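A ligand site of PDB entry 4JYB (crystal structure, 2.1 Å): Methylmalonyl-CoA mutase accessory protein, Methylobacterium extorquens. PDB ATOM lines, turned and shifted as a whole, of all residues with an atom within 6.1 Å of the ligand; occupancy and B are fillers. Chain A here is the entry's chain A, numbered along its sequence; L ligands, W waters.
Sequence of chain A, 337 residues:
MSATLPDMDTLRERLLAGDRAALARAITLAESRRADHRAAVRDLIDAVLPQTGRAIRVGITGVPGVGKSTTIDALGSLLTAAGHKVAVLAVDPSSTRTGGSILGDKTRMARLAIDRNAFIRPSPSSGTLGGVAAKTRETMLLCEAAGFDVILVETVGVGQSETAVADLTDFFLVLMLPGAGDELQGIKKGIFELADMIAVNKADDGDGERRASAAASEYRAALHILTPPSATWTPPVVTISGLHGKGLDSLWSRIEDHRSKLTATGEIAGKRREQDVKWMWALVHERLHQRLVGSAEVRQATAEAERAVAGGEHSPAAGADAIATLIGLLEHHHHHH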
ATOM      1  N   GLY A  62      16.355   0.417  15.184  1.00  0.00           N
ATOM      2  CA  GLY A  62      17.700   0.281  15.744  1.00  0.00           C
ATOM      3  C   GLY A  62      17.627  -0.009  17.226  1.00  0.00           C
ATOM      4  O   GLY A  62      16.708   0.465  17.925  1.00  0.00           O
ATOM      5  N   VAL A  63      18.571  -0.803  17.727  1.00  0.00           N
ATOM      6  CA  VAL A  63      18.641  -1.089  19.168  1.00  0.00           C
ATOM      7  C   VAL A  63      18.748   0.181  20.005  1.00  0.00           C
ATOM      8  O   VAL A  63      19.365   1.146  19.575  1.00  0.00           O
ATOM      9  CB  VAL A  63      19.824  -2.009  19.548  1.00  0.00           C
ATOM     10  CG1 VAL A  63      19.647  -3.368  18.902  1.00  0.00           C
ATOM     11  CG2 VAL A  63      21.181  -1.389  19.149  1.00  0.00           C
ATOM     12  N   PRO A  64      18.168   0.173  21.217  1.00  0.00           N
ATOM     13  CA  PRO A  64      18.354   1.323  22.085  1.00  0.00           C
ATOM     14  C   PRO A  64      19.827   1.621  22.296  1.00  0.00           C
ATOM     15  O   PRO A  64      20.605   0.710  22.575  1.00  0.00           O
ATOM     16  CB  PRO A  64      17.700   0.877  23.400  1.00  0.00           C
ATOM     17  CG  PRO A  64      16.691  -0.164  22.988  1.00  0.00           C
ATOM     18  CD  PRO A  64      17.364  -0.882  21.851  1.00  0.00           C
ATOM     19  N   GLY A  65      20.220   2.878  22.130  1.00  0.00           N
ATOM     20  CA  GLY A  65      21.605   3.302  22.345  1.00  0.00           C
ATOM     21  C   GLY A  65      22.365   3.469  21.041  1.00  0.00           C
ATOM     22  O   GLY A  65      23.461   3.996  21.034  1.00  0.00           O
ATOM     23  N   VAL A  66      21.767   3.044  19.929  1.00  0.00           N
ATOM     24  CA  VAL A  66      22.441   3.125  18.622  1.00  0.00           C
ATOM     25  C   VAL A  66      22.526   4.541  18.078  1.00  0.00           C
ATOM     26  O   VAL A  66      23.339   4.816  17.205  1.00  0.00           O
ATOM     27  CB  VAL A  66      21.703   2.253  17.591  1.00  0.00           C
ATOM     28  CG1 VAL A  66      20.358   2.868  17.204  1.00  0.00           C
ATOM     29  CG2 VAL A  66      22.569   2.027  16.352  1.00  0.00           C
ATOM     30  N   GLY A  67      21.655   5.437  18.535  1.00  0.00           N
ATOM     31  CA  GLY A  67      21.713   6.843  18.091  1.00  0.00           C
ATOM     32  C   GLY A  67      20.584   7.278  17.189  1.00  0.00           C
ATOM     33  O   GLY A  67      20.723   8.206  16.404  1.00  0.00           O
ATOM     34  N   LYS A  68      19.458   6.596  17.339  1.00  0.00           N
ATOM     35  CA  LYS A  68      18.221   6.861  16.632  1.00  0.00           C
ATOM     36  C   LYS A  68      17.637   8.289  16.858  1.00  0.00           C
ATOM     37  O   LYS A  68      17.368   9.003  15.925  1.00  0.00           O
ATOM     38  CB  LYS A  68      17.228   5.761  17.067  1.00  0.00           C
ATOM     39  CG  LYS A  68      16.106   5.412  16.135  1.00  0.00           C
ATOM     40  CD  LYS A  68      15.504   4.039  16.467  1.00  0.00           C
ATOM     41  CE  LYS A  68      15.296   3.763  17.958  1.00  0.00           C
ATOM     42  NZ  LYS A  68      16.514   3.263  18.725  1.00  0.00           N
ATOM     43  N   SER A  69      17.429   8.693  18.097  1.00  0.00           N
ATOM     44  CA  SER A  69      16.883  10.056  18.338  1.00  0.00           C
ATOM     45  C   SER A  69      17.834  11.149  17.883  1.00  0.00           C
ATOM     46  O   SER A  69      17.420  12.152  17.296  1.00  0.00           O
ATOM     47  CB  SER A  69      16.586  10.221  19.804  1.00  0.00           C
ATOM     48  OG  SER A  69      15.597   9.297  20.199  1.00  0.00           O
ATOM     49  N   THR A  70      19.112  10.944  18.133  1.00  0.00           N
ATOM     50  CA  THR A  70      20.155  11.869  17.660  1.00  0.00           C
ATOM     51  C   THR A  70      20.152  11.973  16.145  1.00  0.00           C
ATOM     52  O   THR A  70      20.225  13.055  15.610  1.00  0.00           O
ATOM     53  CB  THR A  70      21.550  11.419  18.130  1.00  0.00           C
ATOM     54  OG1 THR A  70      21.520  11.250  19.545  1.00  0.00           O
ATOM     55  CG2 THR A  70      22.615  12.423  17.781  1.00  0.00           C
ATOM     56  N   THR A  71      20.020  10.841  15.461  1.00  0.00           N
ATOM     57  CA  THR A  71      20.063  10.857  14.009  1.00  0.00           C
ATOM     58  C   THR A  71      18.800  11.493  13.442  1.00  0.00           C
ATOM     59  O   THR A  71      18.846  12.257  12.474  1.00  0.00           O
ATOM     60  CB  THR A  71      20.308   9.441  13.434  1.00  0.00           C
ATOM     61  OG1 THR A  71      21.557   8.924  13.930  1.00  0.00           O
ATOM     62  CG2 THR A  71      20.371   9.502  11.959  1.00  0.00           C
ATOM     63  N   ASP A 105       8.928  11.533  24.914  1.00  0.00           N
ATOM     64  CA  ASP A 105      10.333  11.835  25.187  1.00  0.00           C
ATOM     65  C   ASP A 105      10.916  12.764  24.096  1.00  0.00           C
ATOM     66  O   ASP A 105      10.906  12.403  22.923  1.00  0.00           O
ATOM     67  CB  ASP A 105      11.132  10.521  25.273  1.00  0.00           C
ATOM     68  CG  ASP A 105      12.394  10.642  26.127  1.00  0.00           C
ATOM     69  OD1 ASP A 105      12.894  11.776  26.328  1.00  0.00           O
ATOM     70  OD2 ASP A 105      12.882   9.601  26.606  1.00  0.00           O
ATOM     71  N   ARG A 108      15.843  14.141  23.751  1.00  0.00           N
ATOM     72  CA  ARG A 108      16.611  13.457  22.735  1.00  0.00           C
ATOM     73  C   ARG A 108      16.604  14.168  21.381  1.00  0.00           C
ATOM     74  O   ARG A 108      17.552  14.041  20.605  1.00  0.00           O
ATOM     75  CB  ARG A 108      16.017  12.060  22.593  1.00  0.00           C
ATOM     76  CG  ARG A 108      14.565  12.077  22.139  1.00  0.00           C
ATOM     77  CD  ARG A 108      13.690  11.112  22.905  1.00  0.00           C
ATOM     78  NE  ARG A 108      12.570  10.690  22.060  1.00  0.00           N
ATOM     79  CZ  ARG A 108      12.478   9.525  21.435  1.00  0.00           C
ATOM     80  NH1 ARG A 108      11.417   9.286  20.681  1.00  0.00           N
ATOM     81  NH2 ARG A 108      13.426   8.584  21.548  1.00  0.00           N
ATOM     82  N   GLU A 154       9.292   5.747  14.057  1.00  0.00           N
ATOM     83  CA  GLU A 154      10.317   4.993  14.735  1.00  0.00           C
ATOM     84  C   GLU A 154       9.775   3.941  15.670  1.00  0.00           C
ATOM     85  O   GLU A 154       8.666   4.065  16.220  1.00  0.00           O
ATOM     86  CB  GLU A 154      11.302   5.912  15.448  1.00  0.00           C
ATOM     87  CG  GLU A 154      10.803   6.594  16.688  1.00  0.00           C
ATOM     88  CD  GLU A 154      11.826   7.570  17.248  1.00  0.00           C
ATOM     89  OE1 GLU A 154      13.054   7.372  17.054  1.00  0.00           O
ATOM     90  OE2 GLU A 154      11.382   8.517  17.919  1.00  0.00           O
ATOM     91  N   THR A 155      10.548   2.870  15.792  1.00  0.00           N
ATOM     92  CA  THR A 155      10.270   1.867  16.779  1.00  0.00           C
ATOM     93  C   THR A 155      10.783   2.378  18.119  1.00  0.00           C
ATOM     94  O   THR A 155      11.806   3.078  18.147  1.00  0.00           O
ATOM     95  CB  THR A 155      10.989   0.539  16.449  1.00  0.00           C
ATOM     96  OG1 THR A 155      12.396   0.767  16.287  1.00  0.00           O
ATOM     97  CG2 THR A 155      10.429  -0.071  15.208  1.00  0.00           C
ATOM     98  N   VAL A 156      10.061   2.055  19.192  1.00  0.00           N
ATOM     99  CA  VAL A 156      10.432   2.415  20.563  1.00  0.00           C
ATOM    100  C   VAL A 156      10.667   1.139  21.338  1.00  0.00           C
ATOM    101  O   VAL A 156       9.919   0.184  21.170  1.00  0.00           O
ATOM    102  CB  VAL A 156       9.319   3.188  21.299  1.00  0.00           C
ATOM    103  CG1 VAL A 156       9.762   3.588  22.715  1.00  0.00           C
ATOM    104  CG2 VAL A 156       8.890   4.403  20.503  1.00  0.00           C
ATOM    105  N   GLY A 157      11.699   1.115  22.185  1.00  0.00           N
ATOM    106  CA  GLY A 157      12.014  -0.070  23.006  1.00  0.00           C
ATOM    107  C   GLY A 157      12.525  -1.254  22.215  1.00  0.00           C
ATOM    108  O   GLY A 157      12.893  -1.130  21.042  1.00  0.00           O
ATOM    109  N   ASN A 201      25.985   3.705  12.334  1.00  0.00           N
ATOM    110  CA  ASN A 201      26.030   5.023  12.921  1.00  0.00           C
ATOM    111  C   ASN A 201      27.257   5.094  13.823  1.00  0.00           C
ATOM    112  O   ASN A 201      27.917   4.083  14.046  1.00  0.00           O
ATOM    113  CB  ASN A 201      24.756   5.303  13.719  1.00  0.00           C
ATOM    114  CG  ASN A 201      24.669   6.749  14.240  1.00  0.00           C
ATOM    115  OD1 ASN A 201      25.000   7.698  13.516  1.00  0.00           O
ATOM    116  ND2 ASN A 201      24.261   6.915  15.489  1.00  0.00           N
ATOM    117  N   LYS A 202      27.542   6.286  14.332  1.00  0.00           N
ATOM    118  CA  LYS A 202      28.656   6.522  15.258  1.00  0.00           C
ATOM    119  C   LYS A 202      29.974   6.386  14.510  1.00  0.00           C
ATOM    120  O   LYS A 202      30.970   5.968  15.077  1.00  0.00           O
ATOM    121  CB  LYS A 202      28.586   5.623  16.505  1.00  0.00           C
ATOM    122  CG  LYS A 202      27.258   5.699  17.251  1.00  0.00           C
ATOM    123  CD  LYS A 202      27.385   5.288  18.729  1.00  0.00           C
ATOM    124  CE  LYS A 202      26.008   5.219  19.374  1.00  0.00           C
ATOM    125  NZ  LYS A 202      26.058   5.162  20.848  1.00  0.00           N
ATOM    126  N   ALA A 203      29.960   6.774  13.238  1.00  0.00           N
ATOM    127  CA  ALA A 203      31.129   6.718  12.352  1.00  0.00           C
ATOM    128  C   ALA A 203      31.920   8.026  12.482  1.00  0.00           C
ATOM    129  O   ALA A 203      32.176   8.709  11.499  1.00  0.00           O
ATOM    130  CB  ALA A 203      30.666   6.504  10.914  1.00  0.00           C
ATOM    131  N   ASP A 204      32.296   8.371  13.714  1.00  0.00           N
ATOM    132  CA  ASP A 204      32.869   9.683  14.023  1.00  0.00           C
ATOM    133  C   ASP A 204      34.266   9.778  13.415  1.00  0.00           C
ATOM    134  O   ASP A 204      34.977   8.786  13.322  1.00  0.00           O
ATOM    135  CB  ASP A 204      32.904   9.896  15.543  1.00  0.00           C
ATOM    136  CG  ASP A 204      31.520   9.756  16.205  1.00  0.00           C
ATOM    137  OD1 ASP A 204      30.544   9.353  15.550  1.00  0.00           O
ATOM    138  OD2 ASP A 204      31.380  10.042  17.406  1.00  0.00           O
ATOM    139  N   ILE A 240      27.307   6.665   8.916  1.00  0.00           N
ATOM    140  CA  ILE A 240      26.884   8.009   9.255  1.00  0.00           C
ATOM    141  C   ILE A 240      27.350   8.327  10.658  1.00  0.00           C
ATOM    142  O   ILE A 240      27.744   7.440  11.406  1.00  0.00           O
ATOM    143  CB  ILE A 240      25.337   8.162   9.225  1.00  0.00           C
ATOM    144  CG1 ILE A 240      24.668   7.327  10.359  1.00  0.00           C
ATOM    145  CG2 ILE A 240      24.788   7.768   7.883  1.00  0.00           C
ATOM    146  CD1 ILE A 240      23.156   7.450  10.473  1.00  0.00           C
ATOM    147  N   SER A 241      27.287   9.602  11.023  1.00  0.00           N
ATOM    148  CA  SER A 241      27.356  10.001  12.411  1.00  0.00           C
ATOM    149  C   SER A 241      26.183  10.942  12.666  1.00  0.00           C
ATOM    150  O   SER A 241      26.191  12.069  12.196  1.00  0.00           O
ATOM    151  CB  SER A 241      28.647  10.723  12.738  1.00  0.00           C
ATOM    152  OG  SER A 241      28.572  11.243  14.062  1.00  0.00           O
ATOM    153  N   GLY A 242      25.176  10.455  13.402  1.00  0.00           N
ATOM    154  CA  GLY A 242      24.031  11.251  13.763  1.00  0.00           C
ATOM    155  C   GLY A 242      24.446  12.470  14.549  1.00  0.00           C
ATOM    156  O   GLY A 242      23.988  13.569  14.274  1.00  0.00           O
ATOM    157  N   LEU A 243      25.315  12.261  15.534  1.00  0.00           N
ATOM    158  CA  LEU A 243      25.786  13.326  16.417  1.00  0.00           C
ATOM    159  C   LEU A 243      26.548  14.445  15.685  1.00  0.00           C
ATOM    160  O   LEU A 243      26.282  15.628  15.894  1.00  0.00           O
ATOM    161  CB  LEU A 243      26.675  12.702  17.501  1.00  0.00           C
ATOM    162  CG  LEU A 243      27.196  13.586  18.637  1.00  0.00           C
ATOM    163  CD1 LEU A 243      26.047  14.214  19.415  1.00  0.00           C
ATOM    164  CD2 LEU A 243      28.076  12.739  19.550  1.00  0.00           C
ATOM    165  N   HIS A 244      27.475  14.070  14.803  1.00  0.00           N
ATOM    166  CA  HIS A 244      28.339  15.029  14.113  1.00  0.00           C
ATOM    167  C   HIS A 244      27.883  15.363  12.726  1.00  0.00           C
ATOM    168  O   HIS A 244      28.618  16.016  11.998  1.00  0.00           O
ATOM    169  CB  HIS A 244      29.780  14.531  14.116  1.00  0.00           C
ATOM    170  CG  HIS A 244      30.341  14.309  15.503  1.00  0.00           C
ATOM    171  ND1 HIS A 244      30.386  15.276  16.440  1.00  0.00           N
ATOM    172  CD2 HIS A 244      30.857  13.167  16.112  1.00  0.00           C
ATOM    173  CE1 HIS A 244      30.900  14.791  17.580  1.00  0.00           C
ATOM    174  NE2 HIS A 244      31.196  13.493  17.386  1.00  0.00           N
HETATM  175  P1  LIG L   1      16.314   4.746  22.476  1.00  0.00           P
HETATM  176  O1  LIG L   1      16.225   4.056  23.786  1.00  0.00           O
HETATM  177  O2  LIG L   1      15.784   3.738  21.343  1.00  0.00           O
HETATM  178  O3  LIG L   1      15.378   6.075  22.431  1.00  0.00           O
HETATM  179  N1  LIG L   1      18.012   5.211  22.238  1.00  0.00           N
HETATM  180  P2  LIG L   1      18.546   5.990  20.774  1.00  0.00           P
HETATM  181  O4  LIG L   1      18.740   4.940  19.740  1.00  0.00           O
HETATM  182  O5  LIG L   1      17.551   7.107  20.249  1.00  0.00           O
HETATM  183  O6  LIG L   1      19.980   6.683  21.026  1.00  0.00           O
HETATM  184  P3  LIG L   1      20.221   8.266  21.315  1.00  0.00           P
HETATM  185  O7  LIG L   1      19.970   9.082  20.051  1.00  0.00           O
HETATM  186  O8  LIG L   1      19.547   8.628  22.593  1.00  0.00           O
HETATM  187  O9  LIG L   1      21.801   8.180  21.550  1.00  0.00           O
HETATM  188  C1  LIG L   1      22.310   7.313  22.569  1.00  0.00           C
HETATM  189  C2  LIG L   1      23.697   7.782  22.953  1.00  0.00           C
HETATM  190  O10 LIG L   1      24.581   7.574  21.856  1.00  0.00           O
HETATM  191  C3  LIG L   1      23.727   9.268  23.275  1.00  0.00           C
HETATM  192  O11 LIG L   1      24.701   9.531  24.286  1.00  0.00           O
HETATM  193  C4  LIG L   1      24.165   9.925  21.987  1.00  0.00           C
HETATM  194  O12 LIG L   1      24.900  11.147  22.137  1.00  0.00           O
HETATM  195  C5  LIG L   1      25.074   8.855  21.423  1.00  0.00           C
HETATM  196  N2  LIG L   1      25.147   8.998  19.961  1.00  0.00           N
HETATM  197  C6  LIG L   1      24.145   9.105  19.049  1.00  0.00           C
HETATM  198  N3  LIG L   1      24.650   9.222  17.794  1.00  0.00           N
HETATM  199  C7  LIG L   1      26.004   9.210  17.901  1.00  0.00           C
HETATM  200  C8  LIG L   1      27.156   9.317  16.991  1.00  0.00           C
HETATM  201  O13 LIG L   1      26.984   9.421  15.743  1.00  0.00           O
HETATM  202  N4  LIG L   1      28.391   9.261  17.536  1.00  0.00           N
HETATM  203  C9  LIG L   1      28.578   9.132  18.860  1.00  0.00           C
HETATM  204  N5  LIG L   1      29.807   9.077  19.387  1.00  0.00           N
HETATM  205  N6  LIG L   1      27.569   9.040  19.752  1.00  0.00           N
HETATM  206  C10 LIG L   1      26.297   9.069  19.330  1.00  0.00           C
HETATM  207  O   HOH W   1      30.311   9.428  21.887  1.00  0.00           O
HETATM  208  O   HOH W   2      16.750   8.482  22.882  1.00  0.00           O
HETATM  209  O   HOH W   3      14.112   2.204  22.339  1.00  0.00           O
HETATM  210  O   HOH W   4      14.792   6.984  20.248  1.00  0.00           O
HETATM  211  O   HOH W   5      19.979   5.211  24.548  1.00  0.00           O
HETATM  212  O   HOH W   6      23.307   8.547  26.642  1.00  0.00           O
HETATM  213  O   HOH W   7      25.534  10.083  26.560  1.00  0.00           O
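Water W4 lies within hydrogen-bond range of O3 of the ligand (2.4 Å), OG of Ser 69 (2.4 Å) and NH2 of Arg 108 (2.5 Å). Water W3 bridges an oxygen (O2) of the ligand (2.5 Å) and the backbone NH (N) of Gly 157 (2.7 Å). Water W2 lies within hydrogen-bond range of O3 of the ligand and OG of Ser 69. Water W5 lies within hydrogen-bond range of a nitrogen (N1) of the ligand and the backbone NH of Gly 65.
Val 63 touches the ligand. Pro 64 touches the ligand. Val 66 touches the ligand (N to O4, 3.6 Å). Hydrophobic or aromatic side chains within 4 Å of the ligand: Pro 64, Val 66 and Leu 243. Of the 25 residues printed, 15 come within 4 Å of the ligand. The nearest printed residue that does not touch the ligand is Ala 203 (4.7 Å).
The backbone carbonyl oxygen (O) of Ile 240 lies close to the side-chain amide oxygen (OD1) of Asn 201, 3.5 Å away. The guanidinium group of Arg 108 lies within salt-bridge range of the side-chain carboxylate of Glu 154, 2.9 Å away. The side-chain hydroxyl (OG) of Ser 241 lies within hydrogen-bond range of the backbone NH (N) of His 244 (3.1 Å). The backbone carbonyl oxygen of Ile 240 is in hydrogen-bond range of the backbone NH of Lys 202 (3.2 Å). The guanidinium group of Arg 108 lies within hydrogen-bond range of the backbone carbonyl oxygen of Asp 105 (2.5 Å). ND2 of Asn 201 lies within hydrogen-bond range of O of Val 66 (2.9 Å). A ring nitrogen (NE2) of His 244 sits close to the side-chain carboxylate of Asp 204 (3.5 Å). OG1 of Thr 71 is in hydrogen-bond range of O of Gly 67 (2.7 Å).
ND2 of Asn 201 is in hydrogen-bond range of N3 of the ligand, at 3.3 Å. O5 of the ligand sits at hydrogen-bond distance from N of Ser 69 (2.7 Å). An oxygen (O7) of the ligand sits at hydrogen-bond distance from the side-chain hydroxyl (OG1) of Thr 70 (2.7 Å). The side-chain carboxylate of Asp 204 sits at hydrogen-bond distance from a nitrogen (N5) of the ligand (2.7 Å). O4 of the ligand is in hydrogen-bond range of N of Lys 68 (3.0 Å). N of Lys 202 sits close to O13 of the ligand, 3.5 Å away. N of Leu 243 sits at hydrogen-bond distance from O13 of the ligand. An oxygen (O4) of the ligand is in hydrogen-bond range of the backbone NH (N) of Gly 65. The backbone NH (N) of Thr 70 sits at hydrogen-bond distance from an oxygen (O7) of the ligand, 2.8 Å away. The side-chain hydroxyl of Ser 241 sits at hydrogen-bond distance from an oxygen (O13) of the ligand (2.9 Å). The backbone NH of Gly 67 lies within hydrogen-bond range of an oxygen (O4) of the ligand, at 3.2 Å. N of Gly 242 sits at hydrogen-bond distance from O13 of the ligand, 3.1 Å away. An oxygen (O10) of the ligand lies within hydrogen-bond range of the side-chain amino group (NZ) of Lys 202 (3.0 Å). The guanidinium group of Arg 108 is in salt-bridge range of an oxygen (O3) of the ligand (3.3 Å). The side-chain amino group (NZ) of Lys 68 is in salt-bridge range of an oxygen (O2) of the ligand (2.8 Å). The side-chain hydroxyl (OG) of Ser 69 lies within hydrogen-bond range of an oxygen (O5) of the ligand (2.9 Å).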
